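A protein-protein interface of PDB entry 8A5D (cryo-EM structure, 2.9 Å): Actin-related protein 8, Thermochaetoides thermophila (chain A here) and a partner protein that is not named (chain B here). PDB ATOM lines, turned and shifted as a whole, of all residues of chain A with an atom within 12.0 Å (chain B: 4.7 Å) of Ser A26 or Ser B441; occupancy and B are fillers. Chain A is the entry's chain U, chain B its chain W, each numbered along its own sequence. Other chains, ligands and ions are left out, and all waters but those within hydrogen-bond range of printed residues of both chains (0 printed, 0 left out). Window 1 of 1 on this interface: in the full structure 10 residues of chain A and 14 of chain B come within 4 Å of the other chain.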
ATOM      1  N   THR A  18     -11.082 -17.292  30.974  1.00  0.00           N
ATOM      2  CA  THR A  18      -9.925 -18.219  31.054  1.00  0.00           C
ATOM      3  C   THR A  18      -9.444 -18.631  29.657  1.00  0.00           C
ATOM      4  O   THR A  18     -10.257 -18.806  28.717  1.00  0.00           O
ATOM      5  CB  THR A  18     -10.268 -19.428  31.936  1.00  0.00           C
ATOM      6  OG1 THR A  18      -9.082 -20.221  32.019  1.00  0.00           O
ATOM      7  CG2 THR A  18     -11.433 -20.265  31.440  1.00  0.00           C
ATOM      8  N   ASP A  19      -8.135 -18.828  29.550  1.00  0.00           N
ATOM      9  CA  ASP A  19      -7.445 -19.244  28.305  1.00  0.00           C
ATOM     10  C   ASP A  19      -7.556 -20.772  28.149  1.00  0.00           C
ATOM     11  O   ASP A  19      -7.304 -21.281  27.028  1.00  0.00           O
ATOM     12  CB  ASP A  19      -5.958 -18.850  28.344  1.00  0.00           C
ATOM     13  CG  ASP A  19      -5.618 -17.411  28.726  1.00  0.00           C
ATOM     14  OD1 ASP A  19      -6.386 -16.498  28.352  1.00  0.00           O
ATOM     15  OD2 ASP A  19      -4.557 -17.211  29.376  1.00  0.00           O
ATOM     16  N   ASN A  20      -7.763 -21.502  29.252  1.00  0.00           N
ATOM     17  CA  ASN A  20      -7.580 -22.975  29.362  1.00  0.00           C
ATOM     18  C   ASN A  20      -6.183 -23.409  28.860  1.00  0.00           C
ATOM     19  O   ASN A  20      -6.014 -24.590  28.501  1.00  0.00           O
ATOM     20  CB  ASN A  20      -8.743 -23.682  28.678  1.00  0.00           C
ATOM     21  CG  ASN A  20      -9.984 -23.740  29.533  1.00  0.00           C
ATOM     22  OD1 ASN A  20      -9.956 -24.315  30.620  1.00  0.00           O
ATOM     23  ND2 ASN A  20     -11.079 -23.183  29.033  1.00  0.00           N
ATOM     24  N   GLY A  21      -5.187 -22.518  28.902  1.00  0.00           N
ATOM     25  CA  GLY A  21      -3.799 -22.784  28.478  1.00  0.00           C
ATOM     26  C   GLY A  21      -3.663 -23.099  27.003  1.00  0.00           C
ATOM     27  O   GLY A  21      -2.546 -23.445  26.574  1.00  0.00           O
ATOM     28  N   MET A  22      -4.718 -22.882  26.226  1.00  0.00           N
ATOM     29  CA  MET A  22      -4.756 -23.149  24.767  1.00  0.00           C
ATOM     30  C   MET A  22      -4.025 -22.035  24.004  1.00  0.00           C
ATOM     31  O   MET A  22      -3.950 -20.879  24.490  1.00  0.00           O
ATOM     32  CB  MET A  22      -6.205 -23.175  24.284  1.00  0.00           C
ATOM     33  CG  MET A  22      -7.026 -24.254  24.935  1.00  0.00           C
ATOM     34  SD  MET A  22      -6.469 -25.862  24.326  1.00  0.00           S
ATOM     35  CE  MET A  22      -7.701 -26.946  25.040  1.00  0.00           C
ATOM     36  N   ARG A  23      -3.558 -22.377  22.811  1.00  0.00           N
ATOM     37  CA  ARG A  23      -3.122 -21.416  21.772  1.00  0.00           C
ATOM     38  C   ARG A  23      -4.360 -20.664  21.274  1.00  0.00           C
ATOM     39  O   ARG A  23      -5.482 -21.214  21.474  1.00  0.00           O
ATOM     40  CB  ARG A  23      -2.395 -22.172  20.655  1.00  0.00           C
ATOM     41  CG  ARG A  23      -1.086 -22.796  21.115  1.00  0.00           C
ATOM     42  CD  ARG A  23      -0.273 -23.437  20.002  1.00  0.00           C
ATOM     43  NE  ARG A  23      -0.994 -24.477  19.265  1.00  0.00           N
ATOM     44  CZ  ARG A  23      -1.131 -25.761  19.626  1.00  0.00           C
ATOM     45  NH1 ARG A  23      -0.616 -26.223  20.761  1.00  0.00           N
ATOM     46  NH2 ARG A  23      -1.816 -26.576  18.835  1.00  0.00           N
ATOM     47  N   GLN A  24      -4.155 -19.499  20.619  1.00  0.00           N
ATOM     48  CA  GLN A  24      -5.233 -18.689  19.985  1.00  0.00           C
ATOM     49  C   GLN A  24      -6.130 -19.589  19.134  1.00  0.00           C
ATOM     50  O   GLN A  24      -7.370 -19.424  19.219  1.00  0.00           O
ATOM     51  CB  GLN A  24      -4.711 -17.557  19.100  1.00  0.00           C
ATOM     52  CG  GLN A  24      -5.820 -16.799  18.372  1.00  0.00           C
ATOM     53  CD  GLN A  24      -5.314 -15.550  17.702  1.00  0.00           C
ATOM     54  OE1 GLN A  24      -4.216 -15.056  17.967  1.00  0.00           O
ATOM     55  NE2 GLN A  24      -6.133 -15.026  16.810  1.00  0.00           N
ATOM     56  N   THR A  25      -5.561 -20.478  18.323  1.00  0.00           N
ATOM     57  CA  THR A  25      -6.376 -21.359  17.462  1.00  0.00           C
ATOM     58  C   THR A  25      -5.611 -22.621  17.105  1.00  0.00           C
ATOM     59  O   THR A  25      -4.368 -22.585  16.985  1.00  0.00           O
ATOM     60  CB  THR A  25      -6.876 -20.649  16.198  1.00  0.00           C
ATOM     61  OG1 THR A  25      -7.732 -21.578  15.546  1.00  0.00           O
ATOM     62  CG2 THR A  25      -5.800 -20.227  15.229  1.00  0.00           C
ATOM     63  N   SER A  26      -6.384 -23.679  16.927  1.00  0.00           N
ATOM     64  CA  SER A  26      -5.922 -24.971  16.403  1.00  0.00           C
ATOM     65  C   SER A  26      -5.918 -24.951  14.872  1.00  0.00           C
ATOM     66  O   SER A  26      -5.448 -25.947  14.356  1.00  0.00           O
ATOM     67  CB  SER A  26      -6.766 -26.093  16.965  1.00  0.00           C
ATOM     68  OG  SER A  26      -8.111 -26.005  16.530  1.00  0.00           O
ATOM     69  N   TRP A  27      -6.426 -23.914  14.194  1.00  0.00           N
ATOM     70  CA  TRP A  27      -6.593 -23.910  12.721  1.00  0.00           C
ATOM     71  C   TRP A  27      -5.234 -24.057  12.016  1.00  0.00           C
ATOM     72  O   TRP A  27      -4.313 -23.270  12.291  1.00  0.00           O
ATOM     73  CB  TRP A  27      -7.302 -22.646  12.242  1.00  0.00           C
ATOM     74  CG  TRP A  27      -7.784 -22.828  10.836  1.00  0.00           C
ATOM     75  CD1 TRP A  27      -7.026 -22.843   9.696  1.00  0.00           C
ATOM     76  CD2 TRP A  27      -9.120 -23.227  10.457  1.00  0.00           C
ATOM     77  NE1 TRP A  27      -7.817 -23.154   8.625  1.00  0.00           N
ATOM     78  CE2 TRP A  27      -9.099 -23.406   9.062  1.00  0.00           C
ATOM     79  CE3 TRP A  27     -10.335 -23.393  11.152  1.00  0.00           C
ATOM     80  CZ2 TRP A  27     -10.264 -23.708   8.360  1.00  0.00           C
ATOM     81  CZ3 TRP A  27     -11.483 -23.736  10.466  1.00  0.00           C
ATOM     82  CH2 TRP A  27     -11.433 -23.896   9.082  1.00  0.00           C
ATOM     83  N   PRO A  28      -5.016 -25.107  11.171  1.00  0.00           N
ATOM     84  CA  PRO A  28      -3.672 -25.420  10.666  1.00  0.00           C
ATOM     85  C   PRO A  28      -3.054 -24.359   9.742  1.00  0.00           C
ATOM     86  O   PRO A  28      -3.732 -23.851   8.835  1.00  0.00           O
ATOM     87  CB  PRO A  28      -3.861 -26.719   9.896  1.00  0.00           C
ATOM     88  CG  PRO A  28      -5.106 -27.341  10.484  1.00  0.00           C
ATOM     89  CD  PRO A  28      -5.989 -26.160  10.820  1.00  0.00           C
ATOM     90  N   GLU A  29      -1.792 -24.039  10.018  1.00  0.00           N
ATOM     91  CA  GLU A  29      -1.010 -23.037   9.263  1.00  0.00           C
ATOM     92  C   GLU A  29      -0.016 -23.764   8.337  1.00  0.00           C
ATOM     93  O   GLU A  29       1.123 -24.052   8.736  1.00  0.00           O
ATOM     94  CB  GLU A  29      -0.379 -22.096  10.282  1.00  0.00           C
ATOM     95  CG  GLU A  29       0.356 -20.922   9.659  1.00  0.00           C
ATOM     96  CD  GLU A  29       1.179 -20.084  10.629  1.00  0.00           C
ATOM     97  OE1 GLU A  29       1.241 -20.437  11.832  1.00  0.00           O
ATOM     98  OE2 GLU A  29       1.760 -19.074  10.180  1.00  0.00           O
ATOM     99  N   VAL A  30      -0.419 -23.960   7.092  1.00  0.00           N
ATOM    100  CA  VAL A  30       0.332 -24.685   6.025  1.00  0.00           C
ATOM    101  C   VAL A  30       1.459 -23.782   5.503  1.00  0.00           C
ATOM    102  O   VAL A  30       1.158 -22.630   5.087  1.00  0.00           O
ATOM    103  CB  VAL A  30      -0.640 -25.002   4.877  1.00  0.00           C
ATOM    104  CG1 VAL A  30       0.024 -25.718   3.720  1.00  0.00           C
ATOM    105  CG2 VAL A  30      -1.873 -25.741   5.372  1.00  0.00           C
ATOM    106  N   GLU B  20      -5.388 -30.363  20.773  1.00  0.00           N
ATOM    107  CA  GLU B  20      -6.096 -29.553  21.802  1.00  0.00           C
ATOM    108  C   GLU B  20      -7.507 -30.126  21.957  1.00  0.00           C
ATOM    109  O   GLU B  20      -7.694 -31.024  22.798  1.00  0.00           O
ATOM    110  CB  GLU B  20      -6.044 -28.071  21.436  1.00  0.00           C
ATOM    111  CG  GLU B  20      -4.662 -27.451  21.626  1.00  0.00           C
ATOM    112  CD  GLU B  20      -4.388 -26.119  20.935  1.00  0.00           C
ATOM    113  OE1 GLU B  20      -4.806 -25.945  19.771  1.00  0.00           O
ATOM    114  OE2 GLU B  20      -3.737 -25.256  21.559  1.00  0.00           O
ATOM    115  N   ALA B  38     -14.141 -29.581  13.425  1.00  0.00           N
ATOM    116  CA  ALA B  38     -13.746 -28.163  13.421  1.00  0.00           C
ATOM    117  C   ALA B  38     -12.304 -28.054  12.908  1.00  0.00           C
ATOM    118  O   ALA B  38     -11.518 -29.028  12.993  1.00  0.00           O
ATOM    119  CB  ALA B  38     -13.894 -27.614  14.822  1.00  0.00           C
ATOM    120  N   GLY B  39     -11.898 -26.906  12.428  1.00  0.00           N
ATOM    121  CA  GLY B  39     -10.517 -26.774  11.927  1.00  0.00           C
ATOM    122  C   GLY B  39     -10.360 -27.284  10.513  1.00  0.00           C
ATOM    123  O   GLY B  39      -9.222 -27.505  10.103  1.00  0.00           O
ATOM    124  N   SER B 437     -17.008 -24.418  12.315  1.00  0.00           N
ATOM    125  CA  SER B 437     -15.636 -24.905  12.176  1.00  0.00           C
ATOM    126  C   SER B 437     -14.640 -23.873  12.693  1.00  0.00           C
ATOM    127  O   SER B 437     -13.698 -24.258  13.377  1.00  0.00           O
ATOM    128  CB  SER B 437     -15.360 -25.323  10.747  1.00  0.00           C
ATOM    129  OG  SER B 437     -14.006 -25.737  10.551  1.00  0.00           O
ATOM    130  N   ILE B 438     -14.780 -22.612  12.342  1.00  0.00           N
ATOM    131  CA  ILE B 438     -13.854 -21.530  12.837  1.00  0.00           C
ATOM    132  C   ILE B 438     -14.075 -21.318  14.350  1.00  0.00           C
ATOM    133  O   ILE B 438     -13.117 -21.427  15.083  1.00  0.00           O
ATOM    134  CB  ILE B 438     -14.076 -20.223  12.065  1.00  0.00           C
ATOM    135  CG1 ILE B 438     -13.694 -20.370  10.598  1.00  0.00           C
ATOM    136  CG2 ILE B 438     -13.295 -19.134  12.751  1.00  0.00           C
ATOM    137  CD1 ILE B 438     -14.200 -19.286   9.728  1.00  0.00           C
ATOM    138  N   LEU B 439     -15.329 -21.133  14.782  1.00  0.00           N
ATOM    139  CA  LEU B 439     -15.703 -20.934  16.199  1.00  0.00           C
ATOM    140  C   LEU B 439     -15.087 -22.044  17.060  1.00  0.00           C
ATOM    141  O   LEU B 439     -14.364 -21.729  18.024  1.00  0.00           O
ATOM    142  CB  LEU B 439     -17.238 -20.904  16.320  1.00  0.00           C
ATOM    143  CG  LEU B 439     -17.781 -20.820  17.757  1.00  0.00           C
ATOM    144  CD1 LEU B 439     -17.259 -19.541  18.422  1.00  0.00           C
ATOM    145  CD2 LEU B 439     -19.298 -20.884  17.802  1.00  0.00           C
ATOM    146  N   ALA B 440     -15.415 -23.298  16.798  1.00  0.00           N
ATOM    147  CA  ALA B 440     -15.007 -24.420  17.670  1.00  0.00           C
ATOM    148  C   ALA B 440     -13.492 -24.643  17.585  1.00  0.00           C
ATOM    149  O   ALA B 440     -13.025 -25.580  18.233  1.00  0.00           O
ATOM    150  CB  ALA B 440     -15.787 -25.660  17.310  1.00  0.00           C
ATOM    151  N   SER B 441     -12.749 -23.856  16.812  1.00  0.00           N
ATOM    152  CA  SER B 441     -11.272 -23.940  16.749  1.00  0.00           C
ATOM    153  C   SER B 441     -10.576 -22.762  17.460  1.00  0.00           C
ATOM    154  O   SER B 441      -9.326 -22.780  17.517  1.00  0.00           O
ATOM    155  CB  SER B 441     -10.849 -24.039  15.319  1.00  0.00           C
ATOM    156  OG  SER B 441     -10.831 -22.752  14.732  1.00  0.00           O
ATOM    157  N   LEU B 442     -11.329 -21.811  18.037  1.00  0.00           N
ATOM    158  CA  LEU B 442     -10.794 -20.647  18.808  1.00  0.00           C
ATOM    159  C   LEU B 442     -10.501 -21.057  20.255  1.00  0.00           C
ATOM    160  O   LEU B 442     -11.347 -21.712  20.914  1.00  0.00           O
ATOM    161  CB  LEU B 442     -11.791 -19.492  18.814  1.00  0.00           C
ATOM    162  CG  LEU B 442     -12.173 -18.995  17.438  1.00  0.00           C
ATOM    163  CD1 LEU B 442     -13.083 -17.799  17.543  1.00  0.00           C
ATOM    164  CD2 LEU B 442     -10.907 -18.680  16.664  1.00  0.00           C
ATOM    165  N   GLY B 443      -9.347 -20.649  20.755  1.00  0.00           N
ATOM    166  CA  GLY B 443      -8.913 -21.104  22.082  1.00  0.00           C
ATOM    167  C   GLY B 443      -9.791 -20.507  23.141  1.00  0.00           C
ATOM    168  O   GLY B 443     -10.119 -21.222  24.105  1.00  0.00           O
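Of the printed residues of chain B, Thr A25 touches Ser B441.
Ser A26 touches just these residues of chain B: Glu B20 and Ser B441.
Of the printed residues of chain B, Trp A27 touches Gly B39, Ser B437, Ile B438 and Ser B441.
Of chain A, only Met A22 (3.6 Å), Arg A23 (3.1 Å) and Ser A26 (3.4 Å) come within 4 Å of Glu B20.
Gly B39 touches just these residues of chain A: Trp A27 (3.5 Å) and Pro A28 (3.6 Å).
Ser B437 touches just one residue of chain A: Trp A27.
Ile B438 touches one residue of chain A.
No residue of chain A comes within 4 Å of Leu B439.
The nearest printed residue of chain B that does not touch Ser A26 is Ala B440 (5.2 Å).
Met A22 touches Glu B20.
Gly B443 touches Arg A23 (CA to O, 3.5 Å).
CA of Leu B442 touches O of Gln A24, at 3.7 Å.
Ser A26 touches Glu B20.
CE3 of Trp A27 touches CA of Gly B39, 3.5 Å away.
CZ3 of Trp A27 touches OG of Ser B437, at 3.2 Å.
Ile B438 touches Trp A27 (N to CZ3, 3.96 Å).
OG of Ser B441 touches CE3 of Trp A27 (3.7 Å).
CD of Pro A28 touches O of Gly B39, 3.6 Å away.
The side-chain hydroxyl of Ser B441 lies within hydrogen-bond range of the backbone carbonyl oxygen of Ile B438.
OG of Ser B437 sits at hydrogen-bond distance from N of Gly B39 (3.1 Å).
N of Trp A27 is in hydrogen-bond range of OG1 of Thr A25 (3.0 Å).
The backbone carbonyl oxygen (O) of Gln A24 is in hydrogen-bond range of the backbone NH (N) of Gly B443, 2.8 Å away.
The backbone carbonyl oxygen (O) of Ser B441 is in hydrogen-bond range of the side-chain hydroxyl (OG1) of Thr A25 (2.8 Å).
The guanidinium group (NH2) of Arg A23 lies within salt-bridge range of the side-chain carboxylate (OE1) of Glu B20.
The backbone NH (N) of Ser A26 lies within hydrogen-bond range of the backbone carbonyl oxygen (O) of Ser B441, at 3.1 Å.
Of the 13 printed residues of chain A, 7 touch a printed residue of chain B.
Hydrophobic or aromatic side chains of chain A within 4 Å of the printed part of chain B: Met A22, Trp A27 and Pro A28.
Among the printed residues, 13 pairs touch across the chains.
Among the printed residues, Asp or Glu carboxylates within 4 Å of a Lys or Arg side-chain nitrogen of the other chain: Arg A23 with Glu B20 (3.2 Å).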
